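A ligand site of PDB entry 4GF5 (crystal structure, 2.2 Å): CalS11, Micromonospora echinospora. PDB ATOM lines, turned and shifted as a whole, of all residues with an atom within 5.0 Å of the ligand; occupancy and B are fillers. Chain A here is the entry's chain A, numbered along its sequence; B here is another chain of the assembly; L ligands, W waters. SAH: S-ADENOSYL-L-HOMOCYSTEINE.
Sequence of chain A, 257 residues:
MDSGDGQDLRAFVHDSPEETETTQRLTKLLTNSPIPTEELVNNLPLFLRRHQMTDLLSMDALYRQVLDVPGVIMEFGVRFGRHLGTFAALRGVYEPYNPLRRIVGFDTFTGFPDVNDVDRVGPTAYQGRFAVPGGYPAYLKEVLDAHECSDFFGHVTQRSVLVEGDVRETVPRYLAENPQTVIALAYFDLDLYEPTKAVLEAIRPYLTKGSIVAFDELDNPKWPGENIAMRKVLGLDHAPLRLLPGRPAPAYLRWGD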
ATOM      1  N   GLU A  75      24.116 -23.217   7.559  1.00  0.00           N
ATOM      2  CA  GLU A  75      23.089 -22.834   6.619  1.00  0.00           C
ATOM      3  C   GLU A  75      22.627 -24.052   5.841  1.00  0.00           C
ATOM      4  O   GLU A  75      23.457 -24.823   5.315  1.00  0.00           O
ATOM      5  CB  GLU A  75      23.551 -21.748   5.652  1.00  0.00           C
ATOM      6  CG  GLU A  75      22.408 -21.297   4.712  1.00  0.00           C
ATOM      7  CD  GLU A  75      22.844 -20.290   3.651  1.00  0.00           C
ATOM      8  OE1 GLU A  75      24.045 -20.294   3.264  1.00  0.00           O
ATOM      9  OE2 GLU A  75      21.994 -19.504   3.198  1.00  0.00           O
ATOM     10  N   PHE A  76      21.324 -24.234   5.777  1.00  0.00           N
ATOM     11  CA  PHE A  76      20.764 -25.315   5.004  1.00  0.00           C
ATOM     12  C   PHE A  76      20.149 -24.733   3.730  1.00  0.00           C
ATOM     13  O   PHE A  76      19.109 -24.093   3.774  1.00  0.00           O
ATOM     14  CB  PHE A  76      19.732 -26.086   5.837  1.00  0.00           C
ATOM     15  CG  PHE A  76      20.190 -26.402   7.228  1.00  0.00           C
ATOM     16  CD1 PHE A  76      21.150 -27.376   7.458  1.00  0.00           C
ATOM     17  CD2 PHE A  76      19.643 -25.748   8.326  1.00  0.00           C
ATOM     18  CE1 PHE A  76      21.575 -27.688   8.750  1.00  0.00           C
ATOM     19  CE2 PHE A  76      20.061 -26.057   9.626  1.00  0.00           C
ATOM     20  CZ  PHE A  76      21.026 -27.020   9.828  1.00  0.00           C
ATOM     21  N   GLY A  77      20.813 -24.950   2.603  1.00  0.00           N
ATOM     22  CA  GLY A  77      20.395 -24.322   1.362  1.00  0.00           C
ATOM     23  C   GLY A  77      21.308 -23.137   1.123  1.00  0.00           C
ATOM     24  O   GLY A  77      21.126 -22.075   1.707  1.00  0.00           O
ATOM     25  N   VAL A  78      22.288 -23.342   0.239  1.00  0.00           N
ATOM     26  CA  VAL A  78      23.405 -22.422   0.089  1.00  0.00           C
ATOM     27  C   VAL A  78      23.360 -21.699  -1.255  1.00  0.00           C
ATOM     28  O   VAL A  78      23.816 -20.559  -1.372  1.00  0.00           O
ATOM     29  CB  VAL A  78      24.718 -23.244   0.192  1.00  0.00           C
ATOM     30  CG1 VAL A  78      25.913 -22.470  -0.349  1.00  0.00           C
ATOM     31  CG2 VAL A  78      24.959 -23.669   1.622  1.00  0.00           C
ATOM     32  N   ARG A  79      22.821 -22.378  -2.253  1.00  0.00           N
ATOM     33  CA  ARG A  79      22.879 -21.925  -3.637  1.00  0.00           C
ATOM     34  C   ARG A  79      24.285 -21.458  -4.043  1.00  0.00           C
ATOM     35  O   ARG A  79      25.233 -22.233  -3.958  1.00  0.00           O
ATOM     36  CB  ARG A  79      21.837 -20.838  -3.919  1.00  0.00           C
ATOM     37  CG  ARG A  79      21.439 -20.812  -5.396  1.00  0.00           C
ATOM     38  CD  ARG A  79      20.468 -19.690  -5.710  1.00  0.00           C
ATOM     39  NE  ARG A  79      20.166 -19.649  -7.135  1.00  0.00           N
ATOM     40  CZ  ARG A  79      19.495 -18.649  -7.709  1.00  0.00           C
ATOM     41  NH1 ARG A  79      19.073 -17.641  -6.974  1.00  0.00           N
ATOM     42  NH2 ARG A  79      19.260 -18.675  -9.012  1.00  0.00           N
ATOM     43  N   ARG A  82      26.020 -16.842  -1.159  1.00  0.00           N
ATOM     44  CA  ARG A  82      25.879 -15.480  -0.653  1.00  0.00           C
ATOM     45  C   ARG A  82      26.004 -15.376   0.870  1.00  0.00           C
ATOM     46  O   ARG A  82      26.860 -14.649   1.376  1.00  0.00           O
ATOM     47  CB  ARG A  82      24.523 -14.895  -1.084  1.00  0.00           C
ATOM     48  CG  ARG A  82      24.120 -13.643  -0.305  1.00  0.00           C
ATOM     49  CD  ARG A  82      22.772 -13.104  -0.769  1.00  0.00           C
ATOM     50  NE  ARG A  82      21.665 -14.003  -0.425  1.00  0.00           N
ATOM     51  CZ  ARG A  82      20.378 -13.666  -0.496  1.00  0.00           C
ATOM     52  NH1 ARG A  82      20.055 -12.450  -0.906  1.00  0.00           N
ATOM     53  NH2 ARG A  82      19.435 -14.532  -0.169  1.00  0.00           N
ATOM     54  N   HIS A  83      25.180 -16.116   1.600  1.00  0.00           N
ATOM     55  CA  HIS A  83      25.238 -16.062   3.054  1.00  0.00           C
ATOM     56  C   HIS A  83      26.553 -16.597   3.639  1.00  0.00           C
ATOM     57  O   HIS A  83      27.011 -16.105   4.668  1.00  0.00           O
ATOM     58  CB  HIS A  83      24.043 -16.776   3.671  1.00  0.00           C
ATOM     59  CG  HIS A  83      22.742 -16.081   3.429  1.00  0.00           C
ATOM     60  ND1 HIS A  83      21.530 -16.729   3.448  1.00  0.00           N
ATOM     61  CD2 HIS A  83      22.475 -14.793   3.153  1.00  0.00           C
ATOM     62  CE1 HIS A  83      20.560 -15.871   3.208  1.00  0.00           C
ATOM     63  NE2 HIS A  83      21.108 -14.681   3.032  1.00  0.00           N
ATOM     64  N   PHE A 106      25.142 -26.751   3.757  1.00  0.00           N
ATOM     65  CA  PHE A 106      24.613 -27.980   3.198  1.00  0.00           C
ATOM     66  C   PHE A 106      23.765 -27.657   1.969  1.00  0.00           C
ATOM     67  O   PHE A 106      22.903 -26.781   2.022  1.00  0.00           O
ATOM     68  CB  PHE A 106      23.691 -28.686   4.186  1.00  0.00           C
ATOM     69  CG  PHE A 106      24.351 -29.113   5.475  1.00  0.00           C
ATOM     70  CD1 PHE A 106      24.459 -28.241   6.539  1.00  0.00           C
ATOM     71  CD2 PHE A 106      24.792 -30.419   5.636  1.00  0.00           C
ATOM     72  CE1 PHE A 106      25.030 -28.648   7.731  1.00  0.00           C
ATOM     73  CE2 PHE A 106      25.358 -30.833   6.812  1.00  0.00           C
ATOM     74  CZ  PHE A 106      25.476 -29.943   7.878  1.00  0.00           C
ATOM     75  N   ASP A 107      23.997 -28.392   0.883  1.00  0.00           N
ATOM     76  CA  ASP A 107      23.175 -28.274  -0.322  1.00  0.00           C
ATOM     77  C   ASP A 107      23.454 -29.462  -1.245  1.00  0.00           C
ATOM     78  O   ASP A 107      24.494 -30.116  -1.148  1.00  0.00           O
ATOM     79  CB  ASP A 107      23.475 -26.964  -1.056  1.00  0.00           C
ATOM     80  CG  ASP A 107      22.308 -26.487  -1.901  1.00  0.00           C
ATOM     81  OD1 ASP A 107      21.775 -27.303  -2.670  1.00  0.00           O
ATOM     82  OD2 ASP A 107      21.900 -25.313  -1.797  1.00  0.00           O
ATOM     83  N   THR A 108      22.509 -29.773  -2.130  1.00  0.00           N
ATOM     84  CA  THR A 108      22.780 -30.720  -3.193  1.00  0.00           C
ATOM     85  C   THR A 108      23.726 -30.047  -4.191  1.00  0.00           C
ATOM     86  O   THR A 108      24.591 -30.705  -4.792  1.00  0.00           O
ATOM     87  CB  THR A 108      21.509 -31.164  -3.935  1.00  0.00           C
ATOM     88  OG1 THR A 108      20.876 -30.034  -4.546  1.00  0.00           O
ATOM     89  CG2 THR A 108      20.528 -31.826  -2.986  1.00  0.00           C
ATOM     90  N   PHE A 109      23.565 -28.745  -4.351  1.00  0.00           N
ATOM     91  CA  PHE A 109      24.233 -27.975  -5.405  1.00  0.00           C
ATOM     92  C   PHE A 109      23.774 -28.421  -6.792  1.00  0.00           C
ATOM     93  O   PHE A 109      24.351 -28.035  -7.811  1.00  0.00           O
ATOM     94  CB  PHE A 109      25.750 -28.041  -5.265  1.00  0.00           C
ATOM     95  CG  PHE A 109      26.253 -27.426  -4.004  1.00  0.00           C
ATOM     96  CD1 PHE A 109      26.409 -26.048  -3.900  1.00  0.00           C
ATOM     97  CD2 PHE A 109      26.554 -28.217  -2.907  1.00  0.00           C
ATOM     98  CE1 PHE A 109      26.855 -25.463  -2.735  1.00  0.00           C
ATOM     99  CE2 PHE A 109      27.008 -27.649  -1.729  1.00  0.00           C
ATOM    100  CZ  PHE A 109      27.174 -26.263  -1.645  1.00  0.00           C
ATOM    101  N   THR A 110      22.714 -29.205  -6.827  1.00  0.00           N
ATOM    102  CA  THR A 110      22.097 -29.551  -8.098  1.00  0.00           C
ATOM    103  C   THR A 110      20.607 -29.240  -8.023  1.00  0.00           C
ATOM    104  O   THR A 110      19.814 -29.906  -8.672  1.00  0.00           O
ATOM    105  CB  THR A 110      22.283 -31.030  -8.431  1.00  0.00           C
ATOM    106  OG1 THR A 110      21.527 -31.810  -7.506  1.00  0.00           O
ATOM    107  CG2 THR A 110      23.770 -31.440  -8.381  1.00  0.00           C
ATOM    108  N   GLY A 111      20.234 -28.251  -7.226  1.00  0.00           N
ATOM    109  CA  GLY A 111      18.834 -27.857  -7.086  1.00  0.00           C
ATOM    110  C   GLY A 111      17.991 -28.718  -6.155  1.00  0.00           C
ATOM    111  O   GLY A 111      18.490 -29.672  -5.542  1.00  0.00           O
ATOM    112  N   PHE A 112      16.714 -28.359  -6.047  1.00  0.00           N
ATOM    113  CA  PHE A 112      15.710 -29.175  -5.353  1.00  0.00           C
ATOM    114  C   PHE A 112      15.860 -30.642  -5.749  1.00  0.00           C
ATOM    115  O   PHE A 112      15.911 -30.965  -6.937  1.00  0.00           O
ATOM    116  CB  PHE A 112      14.284 -28.739  -5.742  1.00  0.00           C
ATOM    117  CG  PHE A 112      13.891 -27.377  -5.222  1.00  0.00           C
ATOM    118  CD1 PHE A 112      14.516 -26.808  -4.114  1.00  0.00           C
ATOM    119  CD2 PHE A 112      12.857 -26.665  -5.839  1.00  0.00           C
ATOM    120  CE1 PHE A 112      14.130 -25.557  -3.648  1.00  0.00           C
ATOM    121  CE2 PHE A 112      12.478 -25.416  -5.380  1.00  0.00           C
ATOM    122  CZ  PHE A 112      13.111 -24.861  -4.273  1.00  0.00           C
ATOM    123  N   PRO A 113      15.940 -31.538  -4.755  1.00  0.00           N
ATOM    124  CA  PRO A 113      16.054 -32.972  -5.069  1.00  0.00           C
ATOM    125  C   PRO A 113      14.728 -33.586  -5.515  1.00  0.00           C
ATOM    126  O   PRO A 113      14.726 -34.413  -6.433  1.00  0.00           O
ATOM    127  CB  PRO A 113      16.527 -33.591  -3.742  1.00  0.00           C
ATOM    128  CG  PRO A 113      16.063 -32.648  -2.694  1.00  0.00           C
ATOM    129  CD  PRO A 113      16.022 -31.271  -3.308  1.00  0.00           C
ATOM    130  N   ARG A 129      15.384 -27.103  -9.603  1.00  0.00           N
ATOM    131  CA  ARG A 129      15.280 -25.650  -9.421  1.00  0.00           C
ATOM    132  C   ARG A 129      16.395 -25.124  -8.501  1.00  0.00           C
ATOM    133  O   ARG A 129      16.684 -25.724  -7.464  1.00  0.00           O
ATOM    134  CB  ARG A 129      13.899 -25.269  -8.892  1.00  0.00           C
ATOM    135  CG  ARG A 129      13.709 -23.794  -8.616  1.00  0.00           C
ATOM    136  CD  ARG A 129      13.652 -23.002  -9.912  1.00  0.00           C
ATOM    137  NE  ARG A 129      13.621 -21.569  -9.661  1.00  0.00           N
ATOM    138  CZ  ARG A 129      13.488 -20.639 -10.616  1.00  0.00           C
ATOM    139  NH1 ARG A 129      13.355 -21.010 -11.881  1.00  0.00           N
ATOM    140  NH2 ARG A 129      13.474 -19.356 -10.288  1.00  0.00           N
ATOM    141  N   PHE A 130      17.026 -24.019  -8.905  1.00  0.00           N
ATOM    142  CA  PHE A 130      18.145 -23.386  -8.180  1.00  0.00           C
ATOM    143  C   PHE A 130      19.484 -24.134  -8.284  1.00  0.00           C
ATOM    144  O   PHE A 130      20.416 -23.872  -7.517  1.00  0.00           O
ATOM    145  CB  PHE A 130      17.775 -23.113  -6.706  1.00  0.00           C
ATOM    146  CG  PHE A 130      16.613 -22.169  -6.527  1.00  0.00           C
ATOM    147  CD1 PHE A 130      16.570 -20.951  -7.213  1.00  0.00           C
ATOM    148  CD2 PHE A 130      15.556 -22.492  -5.687  1.00  0.00           C
ATOM    149  CE1 PHE A 130      15.503 -20.084  -7.063  1.00  0.00           C
ATOM    150  CE2 PHE A 130      14.479 -21.631  -5.530  1.00  0.00           C
ATOM    151  CZ  PHE A 130      14.454 -20.424  -6.210  1.00  0.00           C
ATOM    152  N   GLY A 165      25.039 -32.951  -0.857  1.00  0.00           N
ATOM    153  CA  GLY A 165      24.086 -34.039  -0.836  1.00  0.00           C
ATOM    154  C   GLY A 165      22.736 -33.645  -0.255  1.00  0.00           C
ATOM    155  O   GLY A 165      22.467 -32.475  -0.002  1.00  0.00           O
ATOM    156  N   ASP A 166      21.882 -34.644  -0.041  1.00  0.00           N
ATOM    157  CA  ASP A 166      20.543 -34.417   0.467  1.00  0.00           C
ATOM    158  C   ASP A 166      20.589 -34.264   2.002  1.00  0.00           C
ATOM    159  O   ASP A 166      21.006 -35.185   2.697  1.00  0.00           O
ATOM    160  CB  ASP A 166      19.625 -35.572   0.077  1.00  0.00           C
ATOM    161  CG  ASP A 166      18.157 -35.218   0.170  1.00  0.00           C
ATOM    162  OD1 ASP A 166      17.795 -34.425   1.083  1.00  0.00           O
ATOM    163  OD2 ASP A 166      17.379 -35.706  -0.660  1.00  0.00           O
ATOM    164  N   VAL A 167      20.147 -33.100   2.503  1.00  0.00           N
ATOM    165  CA  VAL A 167      20.230 -32.801   3.952  1.00  0.00           C
ATOM    166  C   VAL A 167      19.618 -33.863   4.851  1.00  0.00           C
ATOM    167  O   VAL A 167      20.090 -34.046   5.964  1.00  0.00           O
ATOM    168  CB  VAL A 167      19.603 -31.422   4.317  1.00  0.00           C
ATOM    169  CG1 VAL A 167      20.413 -30.287   3.732  1.00  0.00           C
ATOM    170  CG2 VAL A 167      18.153 -31.338   3.873  1.00  0.00           C
ATOM    171  N   ARG A 168      18.594 -34.564   4.354  1.00  0.00           N
ATOM    172  CA  ARG A 168      17.951 -35.631   5.117  1.00  0.00           C
ATOM    173  C   ARG A 168      18.950 -36.686   5.516  1.00  0.00           C
ATOM    174  O   ARG A 168      18.805 -37.320   6.556  1.00  0.00           O
ATOM    175  CB  ARG A 168      16.823 -36.308   4.317  1.00  0.00           C
ATOM    176  CG  ARG A 168      15.597 -35.456   4.047  1.00  0.00           C
ATOM    177  CD  ARG A 168      15.381 -35.327   2.546  1.00  0.00           C
ATOM    178  NE  ARG A 168      14.024 -35.605   2.139  1.00  0.00           N
ATOM    179  CZ  ARG A 168      13.578 -35.456   0.894  1.00  0.00           C
ATOM    180  NH1 ARG A 168      12.311 -35.723   0.616  1.00  0.00           N
ATOM    181  NH2 ARG A 168      14.394 -35.036  -0.065  1.00  0.00           N
ATOM    182  N   ASP A 189      16.946 -22.311   4.662  1.00  0.00           N
ATOM    183  CA  ASP A 189      16.636 -21.701   3.399  1.00  0.00           C
ATOM    184  C   ASP A 189      16.471 -22.807   2.376  1.00  0.00           C
ATOM    185  O   ASP A 189      16.886 -22.675   1.218  1.00  0.00           O
ATOM    186  CB  ASP A 189      17.793 -20.776   2.993  1.00  0.00           C
ATOM    187  CG  ASP A 189      17.379 -19.726   1.984  1.00  0.00           C
ATOM    188  OD1 ASP A 189      16.206 -19.766   1.537  1.00  0.00           O
ATOM    189  OD2 ASP A 189      18.230 -18.870   1.650  1.00  0.00           O
ATOM    190  N   LEU A 190      15.894 -23.919   2.815  1.00  0.00           N
ATOM    191  CA  LEU A 190      15.659 -25.048   1.918  1.00  0.00           C
ATOM    192  C   LEU A 190      14.392 -24.857   1.065  1.00  0.00           C
ATOM    193  O   LEU A 190      14.284 -25.437  -0.013  1.00  0.00           O
ATOM    194  CB  LEU A 190      15.561 -26.341   2.724  1.00  0.00           C
ATOM    195  CG  LEU A 190      16.843 -26.762   3.448  1.00  0.00           C
ATOM    196  CD1 LEU A 190      16.529 -27.766   4.558  1.00  0.00           C
ATOM    197  CD2 LEU A 190      17.862 -27.344   2.450  1.00  0.00           C
ATOM    198  N   ASP A 191      13.441 -24.061   1.586  1.00  0.00           N
ATOM    199  CA  ASP A 191      12.124 -23.803   0.982  1.00  0.00           C
ATOM    200  C   ASP A 191      11.131 -24.949   1.111  1.00  0.00           C
ATOM    201  O   ASP A 191       9.933 -24.724   1.278  1.00  0.00           O
ATOM    202  CB  ASP A 191      12.207 -23.354  -0.488  1.00  0.00           C
ATOM    203  CG  ASP A 191      12.941 -22.042  -0.665  1.00  0.00           C
ATOM    204  OD1 ASP A 191      13.266 -21.383   0.343  1.00  0.00           O
ATOM    205  OD2 ASP A 191      13.184 -21.679  -1.830  1.00  0.00           O
ATOM    206  N   LEU A 192      11.636 -26.186   1.044  1.00  0.00           N
ATOM    207  CA  LEU A 192      10.794 -27.375   0.963  1.00  0.00           C
ATOM    208  C   LEU A 192      10.416 -28.013   2.307  1.00  0.00           C
ATOM    209  O   LEU A 192      11.201 -28.021   3.254  1.00  0.00           O
ATOM    210  CB  LEU A 192      11.494 -28.429   0.104  1.00  0.00           C
ATOM    211  CG  LEU A 192      11.785 -27.931  -1.311  1.00  0.00           C
ATOM    212  CD1 LEU A 192      12.567 -28.988  -2.098  1.00  0.00           C
ATOM    213  CD2 LEU A 192      10.469 -27.599  -1.993  1.00  0.00           C
ATOM    214  N   PRO A 195      12.644 -31.726   3.713  1.00  0.00           N
ATOM    215  CA  PRO A 195      13.964 -31.526   4.305  1.00  0.00           C
ATOM    216  C   PRO A 195      13.941 -30.583   5.531  1.00  0.00           C
ATOM    217  O   PRO A 195      14.683 -30.794   6.494  1.00  0.00           O
ATOM    218  CB  PRO A 195      14.784 -30.934   3.156  1.00  0.00           C
ATOM    219  CG  PRO A 195      13.796 -30.357   2.214  1.00  0.00           C
ATOM    220  CD  PRO A 195      12.537 -31.161   2.353  1.00  0.00           C
ATOM    221  N   ASN B  43      25.311 -11.865  -5.295  1.00  0.00           N
ATOM    222  CA  ASN B  43      26.249 -12.658  -4.516  1.00  0.00           C
ATOM    223  C   ASN B  43      27.560 -11.932  -4.230  1.00  0.00           C
ATOM    224  O   ASN B  43      28.580 -12.556  -3.995  1.00  0.00           O
ATOM    225  CB  ASN B  43      26.551 -13.979  -5.224  1.00  0.00           C
ATOM    226  CG  ASN B  43      25.332 -14.861  -5.298  1.00  0.00           C
ATOM    227  OD1 ASN B  43      25.081 -15.654  -4.380  1.00  0.00           O
ATOM    228  ND2 ASN B  43      24.561 -14.745  -6.390  1.00  0.00           N
HETATM  229  N   SAH L   1      20.539 -19.387   0.826  1.00  0.00           N
HETATM  230  CA  SAH L   1      20.731 -19.076  -0.586  1.00  0.00           C
HETATM  231  CB  SAH L   1      19.518 -19.504  -1.433  1.00  0.00           C
HETATM  232  CG  SAH L   1      19.102 -20.973  -1.255  1.00  0.00           C
HETATM  233  SD  SAH L   1      18.068 -21.584  -2.624  1.00  0.00           S
HETATM  234  C   SAH L   1      21.126 -17.615  -0.807  1.00  0.00           C
HETATM  235  O   SAH L   1      21.250 -17.128  -1.954  1.00  0.00           O
HETATM  236  OXT SAH L   1      21.350 -16.868   0.153  1.00  0.00           O
HETATM  237  C5' SAH L   1      17.532 -23.042  -1.721  1.00  0.00           C
HETATM  238  C4' SAH L   1      18.563 -24.134  -1.787  1.00  0.00           C
HETATM  239  O4' SAH L   1      18.158 -25.203  -0.938  1.00  0.00           O
HETATM  240  C3' SAH L   1      18.728 -24.704  -3.205  1.00  0.00           C
HETATM  241  O3' SAH L   1      20.055 -24.542  -3.633  1.00  0.00           O
HETATM  242  C2' SAH L   1      18.391 -26.186  -3.049  1.00  0.00           C
HETATM  243  O2' SAH L   1      19.252 -27.018  -3.787  1.00  0.00           O
HETATM  244  C1' SAH L   1      18.539 -26.404  -1.549  1.00  0.00           C
HETATM  245  N9  SAH L   1      17.747 -27.569  -1.102  1.00  0.00           N
HETATM  246  C8  SAH L   1      16.376 -27.734  -1.108  1.00  0.00           C
HETATM  247  N7  SAH L   1      16.117 -28.973  -0.623  1.00  0.00           N
HETATM  248  C5  SAH L   1      17.287 -29.588  -0.316  1.00  0.00           C
HETATM  249  C6  SAH L   1      17.603 -30.845   0.197  1.00  0.00           C
HETATM  250  N6  SAH L   1      16.650 -31.713   0.487  1.00  0.00           N
HETATM  251  N1  SAH L   1      18.939 -31.174   0.403  1.00  0.00           N
HETATM  252  C2  SAH L   1      19.946 -30.274   0.095  1.00  0.00           C
HETATM  253  N3  SAH L   1      19.627 -29.038  -0.427  1.00  0.00           N
HETATM  254  C4  SAH L   1      18.325 -28.705  -0.619  1.00  0.00           C
HETATM  255  O   HOH W   1      19.511 -17.004  -4.234  1.00  0.00           O
HETATM  256  O   HOH W   2      24.175 -18.768   0.945  1.00  0.00           O
HETATM  257  O   HOH W   3      23.580 -17.748  -3.327  1.00  0.00           O
HETATM  258  O   HOH W   4      21.725 -25.953  -5.716  1.00  0.00           O
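OD2 of Asp 189 is in salt-bridge range of N of the ligand (2.5 Å).
The side-chain carboxylate (OD2) of Asp 107 lies within hydrogen-bond range of an oxygen (O3') of the ligand, 2.7 Å away.
A nitrogen (N) of the ligand lies within salt-bridge range of the side-chain carboxylate of Glu 75, 2.8 Å away.
O of Gly 77 is in hydrogen-bond range of N of the ligand (2.9 Å).
OXT of the ligand is in salt-bridge range of NE of Arg 82 (2.9 Å).
OD1 of Asp 166 lies within hydrogen-bond range of N6 of the ligand (3.0 Å).
N of Val 167 is in hydrogen-bond range of N1 of the ligand.
O of Gly 111 lies close to O2' of the ligand (3.3 Å).
An oxygen (OXT) of the ligand lies within hydrogen-bond range of a ring nitrogen (ND1) of His 83 (3.3 Å).
The backbone NH (N) of Thr 108 is in hydrogen-bond range of a nitrogen (N3) of the ligand (3.4 Å).
N of Asp 189 lies within hydrogen-bond range of O of Phe 76 (2.9 Å).
OD1 of Asp 107 is in hydrogen-bond range of OG1 of Thr 108, at 3.4 Å.
The side-chain carboxylate of Asp 107 is in hydrogen-bond range of the backbone NH of Arg 79.
The backbone carbonyl oxygen (O) of Glu 75 lies within hydrogen-bond range of the backbone NH (N) of Phe 106, 3.0 Å away.
The guanidinium group of Arg 168 lies within salt-bridge range of the side-chain carboxylate of Asp 166, 3.1 Å away.
The side-chain hydroxyl (OG1) of Thr 108 sits at hydrogen-bond distance from the backbone carbonyl oxygen (O) of Gly 111 (2.6 Å).
The backbone carbonyl oxygen (O) of Gly 165 sits at hydrogen-bond distance from the backbone NH (N) of Thr 108 (3.4 Å).
N of Phe 112 is in hydrogen-bond range of O of Arg 129 (3.0 Å).
Residues that only touch the ligand: Val 78 (3.5 Å), Arg 79 (3.7 Å), Phe 112 (3.7 Å), Pro 113 (3.4 Å), Phe 130 (3.96 Å), Gly 165 (3.3 Å), Leu 190 (3.3 Å), Leu 192 (3.8 Å) and Pro 195 (3.3 Å).
The nearest printed residue that does not touch the ligand is Arg 168 (4.1 Å).
Water W3 lies within hydrogen-bond range of O of the ligand (2.8 Å), OD1 of Asn 43 of chain B (2.8 Å), N of Arg 82 (3.4 Å) and O of Val 78 (3.4 Å).
Water W1 lies within hydrogen-bond range of the guanidinium group (NH1) of Arg 79 (2.8 Å) and an oxygen (O) of the ligand (2.9 Å).
Water W4 lies within hydrogen-bond range of an oxygen (O3') of the ligand, the backbone carbonyl oxygen of Phe 130, the backbone NH of Gly 111 and the side-chain carboxylate of Asp 107.
Water W2 lies within hydrogen-bond range of OE1 of Glu 75, N of His 83, O of Val 78, N of Arg 82 and OXT of the ligand.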
